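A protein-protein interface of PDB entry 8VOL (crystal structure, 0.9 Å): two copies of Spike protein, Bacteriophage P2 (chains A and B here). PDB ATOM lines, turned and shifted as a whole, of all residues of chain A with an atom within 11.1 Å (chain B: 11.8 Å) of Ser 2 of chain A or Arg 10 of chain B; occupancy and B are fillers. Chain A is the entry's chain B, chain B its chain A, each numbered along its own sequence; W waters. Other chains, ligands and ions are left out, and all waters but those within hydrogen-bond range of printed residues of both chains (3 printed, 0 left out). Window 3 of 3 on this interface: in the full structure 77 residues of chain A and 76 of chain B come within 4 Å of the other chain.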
ATOM      1  N   SER A   2     -21.763  13.861 -21.158  1.00  0.00           N
ATOM      2  CA  SER A   2     -21.072  13.356 -22.338  1.00  0.00           C
ATOM      3  C   SER A   2     -19.918  14.268 -22.739  1.00  0.00           C
ATOM      4  O   SER A   2     -19.730  15.349 -22.169  1.00  0.00           O
ATOM      5  CB  SER A   2     -22.046  13.203 -23.507  1.00  0.00           C
ATOM      6  OG  SER A   2     -23.197  12.473 -23.119  1.00  0.00           O
ATOM      7  N   GLY A   3     -19.150  13.820 -23.728  1.00  0.00           N
ATOM      8  CA  GLY A   3     -17.956  14.519 -24.140  1.00  0.00           C
ATOM      9  C   GLY A   3     -18.245  15.690 -25.053  1.00  0.00           C
ATOM     10  O   GLY A   3     -19.389  16.046 -25.338  1.00  0.00           O
ATOM     11  N   SER A   4     -17.159  16.305 -25.521  1.00  0.00           N
ATOM     12  CA  SER A   4     -17.234  17.448 -26.423  1.00  0.00           C
ATOM     13  C   SER A   4     -16.315  17.256 -27.623  1.00  0.00           C
ATOM     14  O   SER A   4     -15.972  18.227 -28.298  1.00  0.00           O
ATOM     15  CB  SER A   4     -16.891  18.743 -25.695  1.00  0.00           C
ATOM     16  OG  SER A   4     -15.568  18.677 -25.219  1.00  0.00           O
ATOM     17  N   ASP A   5     -15.913  16.020 -27.905  1.00  0.00           N
ATOM     18  CA  ASP A   5     -15.042  15.773 -29.037  1.00  0.00           C
ATOM     19  C   ASP A   5     -15.806  15.904 -30.344  1.00  0.00           C
ATOM     20  O   ASP A   5     -17.036  15.859 -30.386  1.00  0.00           O
ATOM     21  CB  ASP A   5     -14.430  14.385 -28.940  1.00  0.00           C
ATOM     22  CG  ASP A   5     -13.526  14.246 -27.754  1.00  0.00           C
ATOM     23  OD1 ASP A   5     -13.447  13.131 -27.203  1.00  0.00           O
ATOM     24  OD2 ASP A   5     -12.917  15.260 -27.344  1.00  0.00           O
ATOM     25  N   ALA A   6     -15.046  16.055 -31.423  1.00  0.00           N
ATOM     26  CA  ALA A   6     -15.590  16.217 -32.760  1.00  0.00           C
ATOM     27  C   ALA A   6     -14.752  15.401 -33.733  1.00  0.00           C
ATOM     28  O   ALA A   6     -13.557  15.179 -33.513  1.00  0.00           O
ATOM     29  CB  ALA A   6     -15.622  17.695 -33.174  1.00  0.00           C
ATOM     30  N   LEU A   7     -15.389  14.975 -34.818  1.00  0.00           N
ATOM     31  CA  LEU A   7     -14.751  14.145 -35.831  1.00  0.00           C
ATOM     32  C   LEU A   7     -15.209  14.649 -37.188  1.00  0.00           C
ATOM     33  O   LEU A   7     -16.390  14.528 -37.555  1.00  0.00           O
ATOM     34  CB  LEU A   7     -15.122  12.675 -35.646  1.00  0.00           C
ATOM     35  CG  LEU A   7     -14.578  11.694 -36.699  1.00  0.00           C
ATOM     36  CD1 LEU A   7     -13.054  11.644 -36.689  1.00  0.00           C
ATOM     37  CD2 LEU A   7     -15.173  10.310 -36.465  1.00  0.00           C
ATOM     38  N   TYR A  19     -18.566  12.576 -37.939  1.00  0.00           N
ATOM     39  CA  TYR A  19     -19.667  12.278 -37.042  1.00  0.00           C
ATOM     40  C   TYR A  19     -20.449  13.556 -36.802  1.00  0.00           C
ATOM     41  O   TYR A  19     -19.856  14.604 -36.524  1.00  0.00           O
ATOM     42  CB  TYR A  19     -19.216  11.714 -35.708  1.00  0.00           C
ATOM     43  CG  TYR A  19     -20.377  11.179 -34.905  1.00  0.00           C
ATOM     44  CD1 TYR A  19     -21.066  10.057 -35.349  1.00  0.00           C
ATOM     45  CD2 TYR A  19     -20.819  11.793 -33.739  1.00  0.00           C
ATOM     46  CE1 TYR A  19     -22.134   9.548 -34.667  1.00  0.00           C
ATOM     47  CE2 TYR A  19     -21.896  11.286 -33.025  1.00  0.00           C
ATOM     48  CZ  TYR A  19     -22.550  10.153 -33.505  1.00  0.00           C
ATOM     49  OH  TYR A  19     -23.611   9.592 -32.840  1.00  0.00           O
ATOM     50  N   GLU A  20     -21.764  13.469 -36.887  1.00  0.00           N
ATOM     51  CA  GLU A  20     -22.642  14.613 -36.659  1.00  0.00           C
ATOM     52  C   GLU A  20     -23.502  14.281 -35.444  1.00  0.00           C
ATOM     53  O   GLU A  20     -24.414  13.441 -35.539  1.00  0.00           O
ATOM     54  CB  GLU A  20     -23.461  14.886 -37.922  1.00  0.00           C
ATOM     55  CG  GLU A  20     -24.003  16.291 -38.009  1.00  0.00           C
ATOM     56  CD  GLU A  20     -25.003  16.498 -36.919  1.00  0.00           C
ATOM     57  OE1 GLU A  20     -26.105  15.927 -37.033  1.00  0.00           O
ATOM     58  OE2 GLU A  20     -24.673  17.157 -35.911  1.00  0.00           O
ATOM     59  N   PRO A  21     -23.239  14.882 -34.277  1.00  0.00           N
ATOM     60  CA  PRO A  21     -23.941  14.458 -33.058  1.00  0.00           C
ATOM     61  C   PRO A  21     -25.394  14.875 -32.978  1.00  0.00           C
ATOM     62  O   PRO A  21     -26.143  14.250 -32.220  1.00  0.00           O
ATOM     63  CB  PRO A  21     -23.118  15.093 -31.938  1.00  0.00           C
ATOM     64  CG  PRO A  21     -22.528  16.307 -32.572  1.00  0.00           C
ATOM     65  CD  PRO A  21     -22.184  15.864 -33.976  1.00  0.00           C
ATOM     66  N   SER A  24     -26.784  12.144 -34.817  1.00  0.00           N
ATOM     67  CA  SER A  24     -26.069  10.935 -34.417  1.00  0.00           C
ATOM     68  C   SER A  24     -25.710  10.050 -35.611  1.00  0.00           C
ATOM     69  O   SER A  24     -25.897   8.826 -35.594  1.00  0.00           O
ATOM     70  CB  SER A  24     -26.837  10.160 -33.347  1.00  0.00           C
ATOM     71  OG  SER A  24     -27.104  10.932 -32.189  1.00  0.00           O
ATOM     72  N   ALA B   6      -3.322   6.767 -29.659  1.00  0.00           N
ATOM     73  CA  ALA B   6      -4.497   6.392 -28.886  1.00  0.00           C
ATOM     74  C   ALA B   6      -5.745   6.887 -29.592  1.00  0.00           C
ATOM     75  O   ALA B   6      -5.687   7.781 -30.445  1.00  0.00           O
ATOM     76  CB  ALA B   6      -4.436   6.981 -27.468  1.00  0.00           C
ATOM     77  N   LEU B   7      -6.879   6.310 -29.197  1.00  0.00           N
ATOM     78  CA  LEU B   7      -8.173   6.617 -29.799  1.00  0.00           C
ATOM     79  C   LEU B   7      -9.246   6.472 -28.722  1.00  0.00           C
ATOM     80  O   LEU B   7      -9.602   5.354 -28.326  1.00  0.00           O
ATOM     81  CB  LEU B   7      -8.463   5.699 -30.989  1.00  0.00           C
ATOM     82  CG  LEU B   7      -9.834   5.871 -31.641  1.00  0.00           C
ATOM     83  CD1 LEU B   7      -9.974   7.258 -32.242  1.00  0.00           C
ATOM     84  CD2 LEU B   7     -10.087   4.792 -32.705  1.00  0.00           C
ATOM     85  N   HIS B   8      -9.790   7.604 -28.273  1.00  0.00           N
ATOM     86  CA  HIS B   8     -10.942   7.611 -27.372  1.00  0.00           C
ATOM     87  C   HIS B   8     -11.667   8.928 -27.624  1.00  0.00           C
ATOM     88  O   HIS B   8     -11.213   9.972 -27.170  1.00  0.00           O
ATOM     89  CB  HIS B   8     -10.447   7.504 -25.939  1.00  0.00           C
ATOM     90  CG  HIS B   8     -11.534   7.256 -24.945  1.00  0.00           C
ATOM     91  ND1 HIS B   8     -11.430   6.303 -23.956  1.00  0.00           N
ATOM     92  CD2 HIS B   8     -12.754   7.823 -24.795  1.00  0.00           C
ATOM     93  CE1 HIS B   8     -12.536   6.300 -23.233  1.00  0.00           C
ATOM     94  NE2 HIS B   8     -13.356   7.212 -23.723  1.00  0.00           N
ATOM     95  N   ILE B   9     -12.749   8.873 -28.387  1.00  0.00           N
ATOM     96  CA  ILE B   9     -13.525  10.035 -28.798  1.00  0.00           C
ATOM     97  C   ILE B   9     -14.886   9.918 -28.120  1.00  0.00           C
ATOM     98  O   ILE B   9     -15.555   8.885 -28.249  1.00  0.00           O
ATOM     99  CB  ILE B   9     -13.692  10.055 -30.333  1.00  0.00           C
ATOM    100  CG1 ILE B   9     -12.354   9.896 -31.061  1.00  0.00           C
ATOM    101  CG2 ILE B   9     -14.374  11.358 -30.763  1.00  0.00           C
ATOM    102  CD1 ILE B   9     -12.486   9.872 -32.581  1.00  0.00           C
ATOM    103  N   ARG B  10     -15.317  10.971 -27.435  1.00  0.00           N
ATOM    104  CA  ARG B  10     -16.593  11.006 -26.737  1.00  0.00           C
ATOM    105  C   ARG B  10     -17.363  12.215 -27.241  1.00  0.00           C
ATOM    106  O   ARG B  10     -16.955  13.353 -27.004  1.00  0.00           O
ATOM    107  CB  ARG B  10     -16.359  11.092 -25.234  1.00  0.00           C
ATOM    108  CG  ARG B  10     -15.370  10.072 -24.689  1.00  0.00           C
ATOM    109  CD  ARG B  10     -14.965  10.393 -23.245  1.00  0.00           C
ATOM    110  NE  ARG B  10     -16.132  10.499 -22.375  1.00  0.00           N
ATOM    111  CZ  ARG B  10     -16.570  11.620 -21.813  1.00  0.00           C
ATOM    112  NH1 ARG B  10     -15.826  12.714 -21.772  1.00  0.00           N
ATOM    113  NH2 ARG B  10     -17.780  11.638 -21.263  1.00  0.00           N
ATOM    114  N   PHE B  11     -18.454  11.967 -27.933  1.00  0.00           N
ATOM    115  CA  PHE B  11     -19.211  13.003 -28.598  1.00  0.00           C
ATOM    116  C   PHE B  11     -20.307  13.551 -27.699  1.00  0.00           C
ATOM    117  O   PHE B  11     -20.711  12.916 -26.721  1.00  0.00           O
ATOM    118  CB  PHE B  11     -19.834  12.398 -29.846  1.00  0.00           C
ATOM    119  CG  PHE B  11     -18.836  11.951 -30.888  1.00  0.00           C
ATOM    120  CD1 PHE B  11     -18.126  12.860 -31.641  1.00  0.00           C
ATOM    121  CD2 PHE B  11     -18.617  10.599 -31.106  1.00  0.00           C
ATOM    122  CE1 PHE B  11     -17.249  12.424 -32.621  1.00  0.00           C
ATOM    123  CE2 PHE B  11     -17.731  10.172 -32.065  1.00  0.00           C
ATOM    124  CZ  PHE B  11     -17.061  11.081 -32.833  1.00  0.00           C
ATOM    125  N   PRO B  12     -20.830  14.737 -28.034  1.00  0.00           N
ATOM    126  CA  PRO B  12     -21.840  15.379 -27.170  1.00  0.00           C
ATOM    127  C   PRO B  12     -23.148  14.633 -27.024  1.00  0.00           C
ATOM    128  O   PRO B  12     -23.896  14.909 -26.077  1.00  0.00           O
ATOM    129  CB  PRO B  12     -22.059  16.751 -27.840  1.00  0.00           C
ATOM    130  CG  PRO B  12     -20.878  16.985 -28.659  1.00  0.00           C
ATOM    131  CD  PRO B  12     -20.359  15.657 -29.090  1.00  0.00           C
ATOM    132  N   ASP B  13     -23.465  13.727 -27.936  1.00  0.00           N
ATOM    133  CA  ASP B  13     -24.668  12.920 -27.858  1.00  0.00           C
ATOM    134  C   ASP B  13     -24.460  11.621 -27.100  1.00  0.00           C
ATOM    135  O   ASP B  13     -25.378  10.795 -27.061  1.00  0.00           O
ATOM    136  CB  ASP B  13     -25.199  12.609 -29.262  1.00  0.00           C
ATOM    137  CG  ASP B  13     -24.265  11.720 -30.068  1.00  0.00           C
ATOM    138  OD1 ASP B  13     -23.077  11.598 -29.684  1.00  0.00           O
ATOM    139  OD2 ASP B  13     -24.720  11.182 -31.110  1.00  0.00           O
ATOM    140  N   GLY B  14     -23.286  11.422 -26.499  1.00  0.00           N
ATOM    141  CA  GLY B  14     -22.994  10.204 -25.782  1.00  0.00           C
ATOM    142  C   GLY B  14     -22.352   9.113 -26.609  1.00  0.00           C
ATOM    143  O   GLY B  14     -21.961   8.084 -26.048  1.00  0.00           O
ATOM    144  N   ALA B  15     -22.228   9.293 -27.918  1.00  0.00           N
ATOM    145  CA  ALA B  15     -21.567   8.284 -28.740  1.00  0.00           C
ATOM    146  C   ALA B  15     -20.078   8.247 -28.409  1.00  0.00           C
ATOM    147  O   ALA B  15     -19.486   9.250 -27.998  1.00  0.00           O
ATOM    148  CB  ALA B  15     -21.777   8.580 -30.216  1.00  0.00           C
ATOM    149  N   VAL B  16     -19.470   7.081 -28.624  1.00  0.00           N
ATOM    150  CA  VAL B  16     -18.051   6.875 -28.365  1.00  0.00           C
ATOM    151  C   VAL B  16     -17.435   6.083 -29.509  1.00  0.00           C
ATOM    152  O   VAL B  16     -18.044   5.151 -30.046  1.00  0.00           O
ATOM    153  CB  VAL B  16     -17.824   6.153 -27.015  1.00  0.00           C
ATOM    154  CG1 VAL B  16     -16.339   5.901 -26.758  1.00  0.00           C
ATOM    155  CG2 VAL B  16     -18.407   6.959 -25.869  1.00  0.00           C
ATOM    156  N   ILE B  17     -16.206   6.439 -29.859  1.00  0.00           N
ATOM    157  CA  ILE B  17     -15.346   5.629 -30.704  1.00  0.00           C
ATOM    158  C   ILE B  17     -14.057   5.432 -29.922  1.00  0.00           C
ATOM    159  O   ILE B  17     -13.423   6.411 -29.530  1.00  0.00           O
ATOM    160  CB  ILE B  17     -15.070   6.311 -32.052  1.00  0.00           C
ATOM    161  CG1 ILE B  17     -16.365   6.475 -32.850  1.00  0.00           C
ATOM    162  CG2 ILE B  17     -14.014   5.523 -32.837  1.00  0.00           C
ATOM    163  CD1 ILE B  17     -16.216   7.352 -34.089  1.00  0.00           C
ATOM    164  N   GLU B  18     -13.683   4.184 -29.663  1.00  0.00           N
ATOM    165  CA  GLU B  18     -12.544   3.935 -28.798  1.00  0.00           C
ATOM    166  C   GLU B  18     -11.806   2.692 -29.257  1.00  0.00           C
ATOM    167  O   GLU B  18     -12.403   1.745 -29.781  1.00  0.00           O
ATOM    168  CB  GLU B  18     -13.004   3.771 -27.332  1.00  0.00           C
ATOM    169  CG  GLU B  18     -11.927   3.697 -26.274  1.00  0.00           C
ATOM    170  CD  GLU B  18     -11.816   2.339 -25.567  1.00  0.00           C
ATOM    171  OE1 GLU B  18     -12.770   1.524 -25.564  1.00  0.00           O
ATOM    172  OE2 GLU B  18     -10.739   2.095 -24.983  1.00  0.00           O
ATOM    173  N   TYR B  19     -10.498   2.686 -29.034  1.00  0.00           N
ATOM    174  CA  TYR B  19      -9.691   1.491 -29.218  1.00  0.00           C
ATOM    175  C   TYR B  19      -8.949   1.200 -27.924  1.00  0.00           C
ATOM    176  O   TYR B  19      -8.264   2.078 -27.389  1.00  0.00           O
ATOM    177  CB  TYR B  19      -8.692   1.600 -30.370  1.00  0.00           C
ATOM    178  CG  TYR B  19      -8.012   0.275 -30.611  1.00  0.00           C
ATOM    179  CD1 TYR B  19      -8.723  -0.770 -31.174  1.00  0.00           C
ATOM    180  CD2 TYR B  19      -6.714   0.026 -30.192  1.00  0.00           C
ATOM    181  CE1 TYR B  19      -8.158  -2.006 -31.345  1.00  0.00           C
ATOM    182  CE2 TYR B  19      -6.119  -1.218 -30.373  1.00  0.00           C
ATOM    183  CZ  TYR B  19      -6.855  -2.237 -30.955  1.00  0.00           C
ATOM    184  OH  TYR B  19      -6.324  -3.483 -31.170  1.00  0.00           O
ATOM    185  N   THR B  27     -14.332  -0.244 -30.425  1.00  0.00           N
ATOM    186  CA  THR B  27     -15.733  -0.072 -30.066  1.00  0.00           C
ATOM    187  C   THR B  27     -16.268   1.216 -30.672  1.00  0.00           C
ATOM    188  O   THR B  27     -15.678   2.283 -30.512  1.00  0.00           O
ATOM    189  CB  THR B  27     -15.849  -0.024 -28.519  1.00  0.00           C
ATOM    190  OG1 THR B  27     -15.298  -1.215 -27.947  1.00  0.00           O
ATOM    191  CG2 THR B  27     -17.285   0.162 -28.069  1.00  0.00           C
ATOM    192  N   VAL B  28     -17.411   1.113 -31.341  1.00  0.00           N
ATOM    193  CA  VAL B  28     -18.206   2.265 -31.765  1.00  0.00           C
ATOM    194  C   VAL B  28     -19.571   2.058 -31.118  1.00  0.00           C
ATOM    195  O   VAL B  28     -20.194   1.011 -31.320  1.00  0.00           O
ATOM    196  CB  VAL B  28     -18.331   2.327 -33.291  1.00  0.00           C
ATOM    197  CG1 VAL B  28     -19.272   3.454 -33.695  1.00  0.00           C
ATOM    198  CG2 VAL B  28     -16.969   2.450 -33.942  1.00  0.00           C
ATOM    199  N   SER B  29     -20.028   3.014 -30.316  1.00  0.00           N
ATOM    200  CA  SER B  29     -21.276   2.830 -29.598  1.00  0.00           C
ATOM    201  C   SER B  29     -22.047   4.136 -29.536  1.00  0.00           C
ATOM    202  O   SER B  29     -21.489   5.224 -29.683  1.00  0.00           O
ATOM    203  CB  SER B  29     -21.008   2.321 -28.178  1.00  0.00           C
ATOM    204  OG  SER B  29     -20.310   3.306 -27.436  1.00  0.00           O
ATOM    205  N   GLY B  30     -23.354   4.015 -29.295  1.00  0.00           N
ATOM    206  CA  GLY B  30     -24.162   5.177 -28.989  1.00  0.00           C
ATOM    207  C   GLY B  30     -24.552   6.024 -30.166  1.00  0.00           C
ATOM    208  O   GLY B  30     -25.029   7.149 -29.966  1.00  0.00           O
ATOM    209  N   ILE B  31     -24.363   5.526 -31.389  1.00  0.00           N
ATOM    210  CA  ILE B  31     -24.723   6.248 -32.602  1.00  0.00           C
ATOM    211  C   ILE B  31     -26.130   5.840 -33.022  1.00  0.00           C
ATOM    212  O   ILE B  31     -26.672   4.838 -32.542  1.00  0.00           O
ATOM    213  CB  ILE B  31     -23.705   6.003 -33.734  1.00  0.00           C
ATOM    214  CG1 ILE B  31     -23.794   4.581 -34.291  1.00  0.00           C
ATOM    215  CG2 ILE B  31     -22.291   6.352 -33.254  1.00  0.00           C
ATOM    216  CD1 ILE B  31     -22.896   4.338 -35.488  1.00  0.00           C
HETATM  217  O   HOH W   1     -25.745  13.624 -24.266  1.00  0.00           O
HETATM  218  O   HOH W   2     -10.387  12.601 -28.548  1.00  0.00           O
HETATM  219  O   HOH W   3     -27.416   8.511 -30.553  1.00  0.00           O
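The backbone NH of Ser 4 of chain A lies within hydrogen-bond range of the backbone carbonyl oxygen of Arg 10 of chain B, 3.3 Å away. OD2 of Asp 13 of chain B lies within hydrogen-bond range of OG of Ser 24 of chain A (2.6 Å). O of Phe 11 of chain B is in hydrogen-bond range of N of Gly 3 of chain A. OD1 of Asp 5 of chain A sits at hydrogen-bond distance from N of Arg 10 of chain B (2.9 Å). The backbone nitrogen (N) of Pro 12 of chain B lies close to the backbone carbonyl oxygen (O) of Gly 3 of chain A. The side-chain hydroxyl (OH) of Tyr 19 of chain A is in hydrogen-bond range of the side-chain carboxylate (OD2) of Asp 13 of chain B (2.6 Å).
The backbone NH (N) of Ile 9 of chain B is in hydrogen-bond range of the backbone carbonyl oxygen (O) of Ile 17 of chain B, at 2.8 Å. The backbone NH (N) of Ala 15 of chain B lies within hydrogen-bond range of the side-chain carboxylate (OD1) of Asp 13 of chain B (3.0 Å). The backbone NH (N) of Tyr 19 of chain A lies within hydrogen-bond range of the backbone carbonyl oxygen (O) of Leu 7 of chain A, 2.9 Å away. The side-chain hydroxyl of Ser 24 of chain A sits at hydrogen-bond distance from the backbone carbonyl oxygen of Pro 21 of chain A (3.5 Å).
Among the printed residues, pairs that only touch across the chains: Ser 2 of chain A with Arg 10 of chain B (3.7 Å), Ser 2 of chain A with Phe 11 of chain B (3.5 Å), Ser 2 of chain A with Pro 12 of chain B (3.6 Å), Ser 2 of chain A with Gly 14 of chain B (3.5 Å), Gly 3 of chain A with Arg 10 of chain B (3.3 Å), Asp 5 of chain A with His 8 of chain B (3.9 Å), Asp 5 of chain A with Ile 9 of chain B (3.5 Å), Asp 5 of chain A with Phe 11 of chain B (3.4 Å), Asp 5 of chain A with Pro 12 of chain B (3.6 Å), Leu 7 of chain A with Phe 11 of chain B (3.7 Å), Leu 7 of chain A with Ile 17 of chain B (3.9 Å), Tyr 19 of chain A with Phe 11 of chain B (3.5 Å), Tyr 19 of chain A with Ala 15 of chain B (3.4 Å), Tyr 19 of chain A with Ile 31 of chain B (3.5 Å), Pro 21 of chain A with Asp 13 of chain B (3.5 Å) and Ser 24 of chain A with Ile 31 of chain B (3.9 Å).
Gly 3 of chain A touches just these residues of chain B: Arg 10, Phe 11 and Pro 12. Of chain B, only His 8 (3.9 Å), Ile 9 (3.5 Å), Arg 10 (2.9 Å), Phe 11 (3.4 Å) and Pro 12 (3.6 Å) come within 4 Å of Asp 5 of chain A. No residue of chain B comes within 4 Å of Ala 6 of chain A. Printed residues of chain B within 4 Å of Pro 21 of chain A: Asp 13 (3.5 Å). Of the printed residues of chain B, Ser 24 of chain A touches Asp 13 (2.6 Å) and Ile 31 (3.9 Å). Of chain A, only Asp 5 (3.9 Å) comes within 4 Å of His 8 of chain B. Of the printed residues of chain A, Arg 10 of chain B touches Ser 2, Gly 3, Ser 4 and Asp 5. Phe 11 of chain B touches just these residues of chain A: Ser 2 (3.5 Å), Gly 3 (3.5 Å), Asp 5 (3.4 Å), Leu 7 (3.7 Å) and Tyr 19 (3.5 Å). Printed residues of chain A within 4 Å of Pro 12 of chain B: Ser 2, Gly 3 and Asp 5. Of the printed residues of chain A, Asp 13 of chain B touches Tyr 19 (2.6 Å), Pro 21 (3.5 Å) and Ser 24 (2.6 Å). Of chain A, only Ser 2 (3.5 Å) comes within 4 Å of Gly 14 of chain B. Ala 15 of chain B touches just one residue of chain A: Tyr 19 (3.4 Å). Of the printed residues of chain A, Ile 31 of chain B touches Tyr 19 and Ser 24.
Hydrophobic or aromatic side chains of chain A within 4 Å of the printed part of chain B: Leu 7 and Tyr 19. Of the 19 printed residues of chain B, 10 touch a printed residue of chain A. Along chain B the printed residues that touch a printed residue of chain A span positions 8 to 31. Among the printed residues, no Asp or Glu carboxylate lies within 4 Å of a Lys or Arg side-chain nitrogen of the other chain.
Positions printed for both chains: 6, 7 and 19.
Water W3 bridges O of Gly 30 of chain B (2.8 Å) and OG of Ser 24 of chain A (2.9 Å). Water W1 lies within hydrogen-bond range of the backbone carbonyl oxygen of Pro 12 of chain B (2.9 Å) and the side-chain hydroxyl of Ser 2 of chain A (3.0 Å). Water W2 bridges the backbone carbonyl oxygen (O) of His 8 of chain B and the side-chain carboxylate (OD1) of Asp 5 of chain A.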
